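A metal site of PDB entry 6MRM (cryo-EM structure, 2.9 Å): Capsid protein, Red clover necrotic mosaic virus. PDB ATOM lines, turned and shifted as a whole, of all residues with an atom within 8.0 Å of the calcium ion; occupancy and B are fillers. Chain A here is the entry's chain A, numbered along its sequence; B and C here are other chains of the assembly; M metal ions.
The calcium ion is bound by OD1 of Asp 97 of chain B (2.1 Å), NE2 of Gln 211 of chain B (2.1 Å), OD2 of Asp 127 (2.3 Å), OD1 of Asp 130 (2.3 Å) and OD2 of Asp 130 (2.6 Å). Slightly farther from the calcium ion lies OD2 of Asp 97 of chain B (2.9 Å).
Merely in contact with the calcium ion: Asp 169 of chain B (3.5 Å). Of the 26 residues printed, 5 come within 4 Å of the calcium ion.
OE1 of Gln 211 of chain B lies close to O of Tyr 96 of chain B, at 2.9 Å. OE1 of Gln 211 of chain B lies close to OD2 of Asp 169 of chain B, at 3.3 Å. O of Gly 209 of chain B is in hydrogen-bond range of N of Asp 97 of chain B, 3.3 Å away. The backbone NH (N) of Val 167 of chain B is in hydrogen-bond range of the backbone carbonyl oxygen (O) of Asp 97 of chain B (3.0 Å). N of Gln 211 of chain B lies within hydrogen-bond range of O of Asn 95 of chain B (2.7 Å).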
ATOM      1  N   ASP A 125      -7.370 -35.240 -25.671  1.00  0.00           N
ATOM      2  CA  ASP A 125      -7.115 -33.800 -25.681  1.00  0.00           C
ATOM      3  C   ASP A 125      -6.586 -33.328 -24.347  1.00  0.00           C
ATOM      4  O   ASP A 125      -6.914 -33.876 -23.298  1.00  0.00           O
ATOM      5  CB  ASP A 125      -8.363 -33.013 -26.011  1.00  0.00           C
ATOM      6  CG  ASP A 125      -8.401 -32.560 -27.424  1.00  0.00           C
ATOM      7  OD1 ASP A 125      -7.318 -32.212 -27.936  1.00  0.00           O
ATOM      8  OD2 ASP A 125      -9.482 -32.518 -28.041  1.00  0.00           O
ATOM      9  N   PRO A 126      -5.760 -32.309 -24.344  1.00  0.00           N
ATOM     10  CA  PRO A 126      -5.457 -31.607 -23.105  1.00  0.00           C
ATOM     11  C   PRO A 126      -6.510 -30.540 -22.822  1.00  0.00           C
ATOM     12  O   PRO A 126      -6.720 -30.167 -21.667  1.00  0.00           O
ATOM     13  CB  PRO A 126      -4.082 -31.012 -23.360  1.00  0.00           C
ATOM     14  CG  PRO A 126      -4.022 -30.834 -24.813  1.00  0.00           C
ATOM     15  CD  PRO A 126      -4.805 -31.956 -25.413  1.00  0.00           C
ATOM     16  N   ASP A 127      -7.161 -30.044 -23.871  1.00  0.00           N
ATOM     17  CA  ASP A 127      -8.365 -29.258 -23.678  1.00  0.00           C
ATOM     18  C   ASP A 127      -9.503 -30.138 -23.207  1.00  0.00           C
ATOM     19  O   ASP A 127      -9.463 -31.366 -23.319  1.00  0.00           O
ATOM     20  CB  ASP A 127      -8.803 -28.579 -24.973  1.00  0.00           C
ATOM     21  CG  ASP A 127      -8.174 -27.239 -25.175  1.00  0.00           C
ATOM     22  OD1 ASP A 127      -7.959 -26.562 -24.159  1.00  0.00           O
ATOM     23  OD2 ASP A 127      -7.917 -26.854 -26.323  1.00  0.00           O
ATOM     24  N   SER A 128     -10.536 -29.498 -22.704  1.00  0.00           N
ATOM     25  CA  SER A 128     -11.802 -30.174 -22.462  1.00  0.00           C
ATOM     26  C   SER A 128     -12.938 -29.471 -23.176  1.00  0.00           C
ATOM     27  O   SER A 128     -14.108 -29.782 -22.908  1.00  0.00           O
ATOM     28  CB  SER A 128     -12.083 -30.283 -20.970  1.00  0.00           C
ATOM     29  OG  SER A 128     -12.270 -29.002 -20.405  1.00  0.00           O
ATOM     30  N   GLN A 129     -12.630 -28.537 -24.074  1.00  0.00           N
ATOM     31  CA  GLN A 129     -13.637 -27.806 -24.803  1.00  0.00           C
ATOM     32  C   GLN A 129     -13.370 -27.753 -26.294  1.00  0.00           C
ATOM     33  O   GLN A 129     -14.033 -26.988 -26.999  1.00  0.00           O
ATOM     34  CB  GLN A 129     -13.773 -26.384 -24.268  1.00  0.00           C
ATOM     35  CG  GLN A 129     -14.343 -26.293 -22.893  1.00  0.00           C
ATOM     36  CD  GLN A 129     -14.367 -24.890 -22.383  1.00  0.00           C
ATOM     37  OE1 GLN A 129     -13.873 -23.975 -23.032  1.00  0.00           O
ATOM     38  NE2 GLN A 129     -14.951 -24.695 -21.210  1.00  0.00           N
ATOM     39  N   ASP A 130     -12.395 -28.506 -26.798  1.00  0.00           N
ATOM     40  CA  ASP A 130     -12.228 -28.609 -28.240  1.00  0.00           C
ATOM     41  C   ASP A 130     -13.393 -29.377 -28.844  1.00  0.00           C
ATOM     42  O   ASP A 130     -14.077 -30.152 -28.175  1.00  0.00           O
ATOM     43  CB  ASP A 130     -10.920 -29.306 -28.600  1.00  0.00           C
ATOM     44  CG  ASP A 130      -9.714 -28.423 -28.378  1.00  0.00           C
ATOM     45  OD1 ASP A 130      -9.865 -27.192 -28.391  1.00  0.00           O
ATOM     46  OD2 ASP A 130      -8.606 -28.975 -28.219  1.00  0.00           O
ATOM     47  N   SER A 131     -13.616 -29.155 -30.129  1.00  0.00           N
ATOM     48  CA  SER A 131     -14.720 -29.803 -30.823  1.00  0.00           C
ATOM     49  C   SER A 131     -14.318 -31.221 -31.216  1.00  0.00           C
ATOM     50  O   SER A 131     -13.220 -31.688 -30.919  1.00  0.00           O
ATOM     51  CB  SER A 131     -15.133 -28.977 -32.029  1.00  0.00           C
ATOM     52  OG  SER A 131     -14.103 -28.943 -32.987  1.00  0.00           O
ATOM     53  N   TYR A 142      -3.651 -35.794 -32.600  1.00  0.00           N
ATOM     54  CA  TYR A 142      -3.715 -35.410 -31.210  1.00  0.00           C
ATOM     55  C   TYR A 142      -2.410 -35.747 -30.507  1.00  0.00           C
ATOM     56  O   TYR A 142      -1.502 -36.344 -31.086  1.00  0.00           O
ATOM     57  CB  TYR A 142      -4.904 -36.079 -30.535  1.00  0.00           C
ATOM     58  CG  TYR A 142      -6.220 -35.473 -30.924  1.00  0.00           C
ATOM     59  CD1 TYR A 142      -6.717 -34.388 -30.237  1.00  0.00           C
ATOM     60  CD2 TYR A 142      -6.954 -35.956 -31.986  1.00  0.00           C
ATOM     61  CE1 TYR A 142      -7.919 -33.818 -30.580  1.00  0.00           C
ATOM     62  CE2 TYR A 142      -8.163 -35.399 -32.329  1.00  0.00           C
ATOM     63  CZ  TYR A 142      -8.636 -34.327 -31.621  1.00  0.00           C
ATOM     64  OH  TYR A 142      -9.838 -33.757 -31.964  1.00  0.00           O
ATOM     65  N   LYS A 176     -12.516 -25.916 -19.219  1.00  0.00           N
ATOM     66  CA  LYS A 176     -11.175 -25.919 -19.773  1.00  0.00           C
ATOM     67  C   LYS A 176     -10.094 -25.810 -18.719  1.00  0.00           C
ATOM     68  O   LYS A 176      -8.974 -26.288 -18.942  1.00  0.00           O
ATOM     69  CB  LYS A 176     -11.112 -24.760 -20.756  1.00  0.00           C
ATOM     70  CG  LYS A 176      -9.951 -24.684 -21.680  1.00  0.00           C
ATOM     71  CD  LYS A 176     -10.247 -23.584 -22.667  1.00  0.00           C
ATOM     72  CE  LYS A 176      -9.186 -23.470 -23.716  1.00  0.00           C
ATOM     73  NZ  LYS A 176      -9.531 -22.417 -24.694  1.00  0.00           N
ATOM     74  N   ALA B  93       0.433 -21.536 -33.852  1.00  0.00           N
ATOM     75  CA  ALA B  93      -0.430 -21.689 -32.694  1.00  0.00           C
ATOM     76  C   ALA B  93      -1.660 -22.520 -32.999  1.00  0.00           C
ATOM     77  O   ALA B  93      -2.314 -22.983 -32.066  1.00  0.00           O
ATOM     78  CB  ALA B  93      -0.860 -20.328 -32.181  1.00  0.00           C
ATOM     79  N   ALA B  94      -1.980 -22.725 -34.269  1.00  0.00           N
ATOM     80  CA  ALA B  94      -3.121 -23.571 -34.580  1.00  0.00           C
ATOM     81  C   ALA B  94      -2.843 -25.036 -34.327  1.00  0.00           C
ATOM     82  O   ALA B  94      -3.784 -25.827 -34.250  1.00  0.00           O
ATOM     83  CB  ALA B  94      -3.542 -23.363 -36.034  1.00  0.00           C
ATOM     84  N   ASN B  95      -1.587 -25.418 -34.196  1.00  0.00           N
ATOM     85  CA  ASN B  95      -1.232 -26.821 -34.001  1.00  0.00           C
ATOM     86  C   ASN B  95      -1.214 -27.247 -32.549  1.00  0.00           C
ATOM     87  O   ASN B  95      -1.086 -28.434 -32.278  1.00  0.00           O
ATOM     88  CB  ASN B  95       0.130 -27.122 -34.597  1.00  0.00           C
ATOM     89  CG  ASN B  95       0.127 -27.079 -36.080  1.00  0.00           C
ATOM     90  OD1 ASN B  95      -0.820 -27.498 -36.712  1.00  0.00           O
ATOM     91  ND2 ASN B  95       1.216 -26.605 -36.665  1.00  0.00           N
ATOM     92  N   TYR B  96      -1.305 -26.321 -31.602  1.00  0.00           N
ATOM     93  CA  TYR B  96      -1.003 -26.641 -30.220  1.00  0.00           C
ATOM     94  C   TYR B  96      -2.114 -26.137 -29.327  1.00  0.00           C
ATOM     95  O   TYR B  96      -3.008 -25.401 -29.751  1.00  0.00           O
ATOM     96  CB  TYR B  96       0.325 -26.038 -29.817  1.00  0.00           C
ATOM     97  CG  TYR B  96       1.496 -26.583 -30.587  1.00  0.00           C
ATOM     98  CD1 TYR B  96       2.085 -27.781 -30.226  1.00  0.00           C
ATOM     99  CD2 TYR B  96       2.002 -25.897 -31.661  1.00  0.00           C
ATOM    100  CE1 TYR B  96       3.152 -28.271 -30.921  1.00  0.00           C
ATOM    101  CE2 TYR B  96       3.070 -26.387 -32.366  1.00  0.00           C
ATOM    102  CZ  TYR B  96       3.634 -27.572 -31.997  1.00  0.00           C
ATOM    103  OH  TYR B  96       4.702 -28.062 -32.702  1.00  0.00           O
ATOM    104  N   ASP B  97      -2.056 -26.536 -28.055  1.00  0.00           N
ATOM    105  CA  ASP B  97      -3.035 -26.093 -27.074  1.00  0.00           C
ATOM    106  C   ASP B  97      -2.442 -25.479 -25.831  1.00  0.00           C
ATOM    107  O   ASP B  97      -3.198 -24.962 -25.013  1.00  0.00           O
ATOM    108  CB  ASP B  97      -3.944 -27.261 -26.667  1.00  0.00           C
ATOM    109  CG  ASP B  97      -5.105 -27.432 -27.604  1.00  0.00           C
ATOM    110  OD1 ASP B  97      -5.603 -26.409 -28.107  1.00  0.00           O
ATOM    111  OD2 ASP B  97      -5.537 -28.579 -27.838  1.00  0.00           O
ATOM    112  N   MET B  98      -1.128 -25.517 -25.645  1.00  0.00           N
ATOM    113  CA  MET B  98      -0.499 -24.906 -24.490  1.00  0.00           C
ATOM    114  C   MET B  98       0.647 -24.055 -24.980  1.00  0.00           C
ATOM    115  O   MET B  98       1.347 -24.447 -25.913  1.00  0.00           O
ATOM    116  CB  MET B  98       0.023 -25.957 -23.514  1.00  0.00           C
ATOM    117  CG  MET B  98      -0.967 -27.003 -23.083  1.00  0.00           C
ATOM    118  SD  MET B  98      -2.358 -26.375 -22.164  1.00  0.00           S
ATOM    119  CE  MET B  98      -1.608 -26.068 -20.587  1.00  0.00           C
ATOM    120  N   PHE B 166      -3.564 -21.983 -21.868  1.00  0.00           N
ATOM    121  CA  PHE B 166      -4.252 -22.539 -23.017  1.00  0.00           C
ATOM    122  C   PHE B 166      -4.254 -21.585 -24.198  1.00  0.00           C
ATOM    123  O   PHE B 166      -4.333 -20.369 -24.047  1.00  0.00           O
ATOM    124  CB  PHE B 166      -5.684 -22.895 -22.649  1.00  0.00           C
ATOM    125  CG  PHE B 166      -5.787 -24.081 -21.777  1.00  0.00           C
ATOM    126  CD1 PHE B 166      -5.733 -25.339 -22.319  1.00  0.00           C
ATOM    127  CD2 PHE B 166      -5.915 -23.958 -20.414  1.00  0.00           C
ATOM    128  CE1 PHE B 166      -5.834 -26.454 -21.529  1.00  0.00           C
ATOM    129  CE2 PHE B 166      -6.007 -25.070 -19.613  1.00  0.00           C
ATOM    130  CZ  PHE B 166      -5.965 -26.322 -20.175  1.00  0.00           C
ATOM    131  N   VAL B 167      -4.159 -22.162 -25.383  1.00  0.00           N
ATOM    132  CA  VAL B 167      -4.267 -21.400 -26.616  1.00  0.00           C
ATOM    133  C   VAL B 167      -5.741 -21.270 -26.961  1.00  0.00           C
ATOM    134  O   VAL B 167      -6.466 -22.271 -27.000  1.00  0.00           O
ATOM    135  CB  VAL B 167      -3.483 -22.076 -27.739  1.00  0.00           C
ATOM    136  CG1 VAL B 167      -3.640 -21.320 -29.024  1.00  0.00           C
ATOM    137  CG2 VAL B 167      -2.032 -22.169 -27.366  1.00  0.00           C
ATOM    138  N   ALA B 168      -6.186 -20.044 -27.206  1.00  0.00           N
ATOM    139  CA  ALA B 168      -7.619 -19.769 -27.312  1.00  0.00           C
ATOM    140  C   ALA B 168      -8.162 -20.265 -28.646  1.00  0.00           C
ATOM    141  O   ALA B 168      -7.996 -19.600 -29.675  1.00  0.00           O
ATOM    142  CB  ALA B 168      -7.867 -18.279 -27.154  1.00  0.00           C
ATOM    143  N   ASP B 169      -8.844 -21.408 -28.641  1.00  0.00           N
ATOM    144  CA  ASP B 169      -9.630 -21.848 -29.796  1.00  0.00           C
ATOM    145  C   ASP B 169     -11.058 -22.031 -29.292  1.00  0.00           C
ATOM    146  O   ASP B 169     -11.548 -23.164 -29.208  1.00  0.00           O
ATOM    147  CB  ASP B 169      -9.082 -23.143 -30.376  1.00  0.00           C
ATOM    148  CG  ASP B 169      -7.683 -23.001 -30.900  1.00  0.00           C
ATOM    149  OD1 ASP B 169      -7.327 -21.901 -31.349  1.00  0.00           O
ATOM    150  OD2 ASP B 169      -6.933 -24.003 -30.857  1.00  0.00           O
ATOM    151  N   ASN B 170     -11.746 -20.917 -29.094  1.00  0.00           N
ATOM    152  CA  ASN B 170     -12.935 -20.827 -28.275  1.00  0.00           C
ATOM    153  C   ASN B 170     -13.209 -19.324 -28.389  1.00  0.00           C
ATOM    154  O   ASN B 170     -12.359 -18.652 -28.978  1.00  0.00           O
ATOM    155  CB  ASN B 170     -12.539 -21.317 -26.887  1.00  0.00           C
ATOM    156  CG  ASN B 170     -13.563 -22.273 -26.289  1.00  0.00           C
ATOM    157  OD1 ASN B 170     -14.594 -22.528 -26.888  1.00  0.00           O
ATOM    158  ND2 ASN B 170     -13.247 -22.816 -25.123  1.00  0.00           N
ATOM    159  N   GLY B 209       1.666 -29.723 -25.667  1.00  0.00           N
ATOM    160  CA  GLY B 209       1.016 -30.738 -26.494  1.00  0.00           C
ATOM    161  C   GLY B 209       0.205 -30.349 -27.708  1.00  0.00           C
ATOM    162  O   GLY B 209      -0.606 -29.426 -27.682  1.00  0.00           O
ATOM    163  N   PRO B 210       0.407 -31.078 -28.795  1.00  0.00           N
ATOM    164  CA  PRO B 210      -0.176 -30.674 -30.080  1.00  0.00           C
ATOM    165  C   PRO B 210      -1.653 -30.958 -30.236  1.00  0.00           C
ATOM    166  O   PRO B 210      -2.317 -31.393 -29.294  1.00  0.00           O
ATOM    167  CB  PRO B 210       0.645 -31.481 -31.089  1.00  0.00           C
ATOM    168  CG  PRO B 210       1.068 -32.656 -30.365  1.00  0.00           C
ATOM    169  CD  PRO B 210       1.314 -32.227 -28.953  1.00  0.00           C
ATOM    170  N   GLN B 211      -2.164 -30.728 -31.444  1.00  0.00           N
ATOM    171  CA  GLN B 211      -3.584 -30.611 -31.707  1.00  0.00           C
ATOM    172  C   GLN B 211      -3.775 -30.700 -33.204  1.00  0.00           C
ATOM    173  O   GLN B 211      -2.874 -30.311 -33.956  1.00  0.00           O
ATOM    174  CB  GLN B 211      -4.113 -29.270 -31.197  1.00  0.00           C
ATOM    175  CG  GLN B 211      -5.617 -29.124 -31.113  1.00  0.00           C
ATOM    176  CD  GLN B 211      -6.032 -27.715 -30.871  1.00  0.00           C
ATOM    177  OE1 GLN B 211      -5.236 -26.792 -30.967  1.00  0.00           O
ATOM    178  NE2 GLN B 211      -7.300 -27.519 -30.508  1.00  0.00           N
ATOM    179  N   PRO B 212      -4.905 -31.223 -33.682  1.00  0.00           N
ATOM    180  CA  PRO B 212      -5.262 -30.994 -35.073  1.00  0.00           C
ATOM    181  C   PRO B 212      -5.526 -29.512 -35.296  1.00  0.00           C
ATOM    182  O   PRO B 212      -5.986 -28.807 -34.399  1.00  0.00           O
ATOM    183  CB  PRO B 212      -6.529 -31.821 -35.259  1.00  0.00           C
ATOM    184  CG  PRO B 212      -7.046 -32.029 -33.915  1.00  0.00           C
ATOM    185  CD  PRO B 212      -5.848 -32.142 -33.041  1.00  0.00           C
ATOM    186  N   ALA B 214      -6.373 -25.836 -35.891  1.00  0.00           N
ATOM    187  CA  ALA B 214      -7.521 -24.944 -35.868  1.00  0.00           C
ATOM    188  C   ALA B 214      -7.632 -24.260 -37.219  1.00  0.00           C
ATOM    189  O   ALA B 214      -6.627 -23.854 -37.795  1.00  0.00           O
ATOM    190  CB  ALA B 214      -7.376 -23.918 -34.752  1.00  0.00           C
ATOM    191  N   LYS C 331     -12.587 -25.153 -42.104  1.00  0.00           N
ATOM    192  CA  LYS C 331     -13.172 -26.109 -41.177  1.00  0.00           C
ATOM    193  C   LYS C 331     -14.685 -26.134 -41.411  1.00  0.00           C
ATOM    194  O   LYS C 331     -15.199 -25.615 -42.405  1.00  0.00           O
ATOM    195  CB  LYS C 331     -12.812 -25.780 -39.738  1.00  0.00           C
ATOM    196  CG  LYS C 331     -11.366 -26.055 -39.410  1.00  0.00           C
ATOM    197  CD  LYS C 331     -11.068 -25.694 -37.974  1.00  0.00           C
ATOM    198  CE  LYS C 331     -11.711 -26.667 -37.029  1.00  0.00           C
ATOM    199  NZ  LYS C 331     -11.326 -26.416 -35.627  1.00  0.00           N
HETATM  200 CA    CA M   1      -7.623 -26.631 -28.578  1.00  0.00          CA
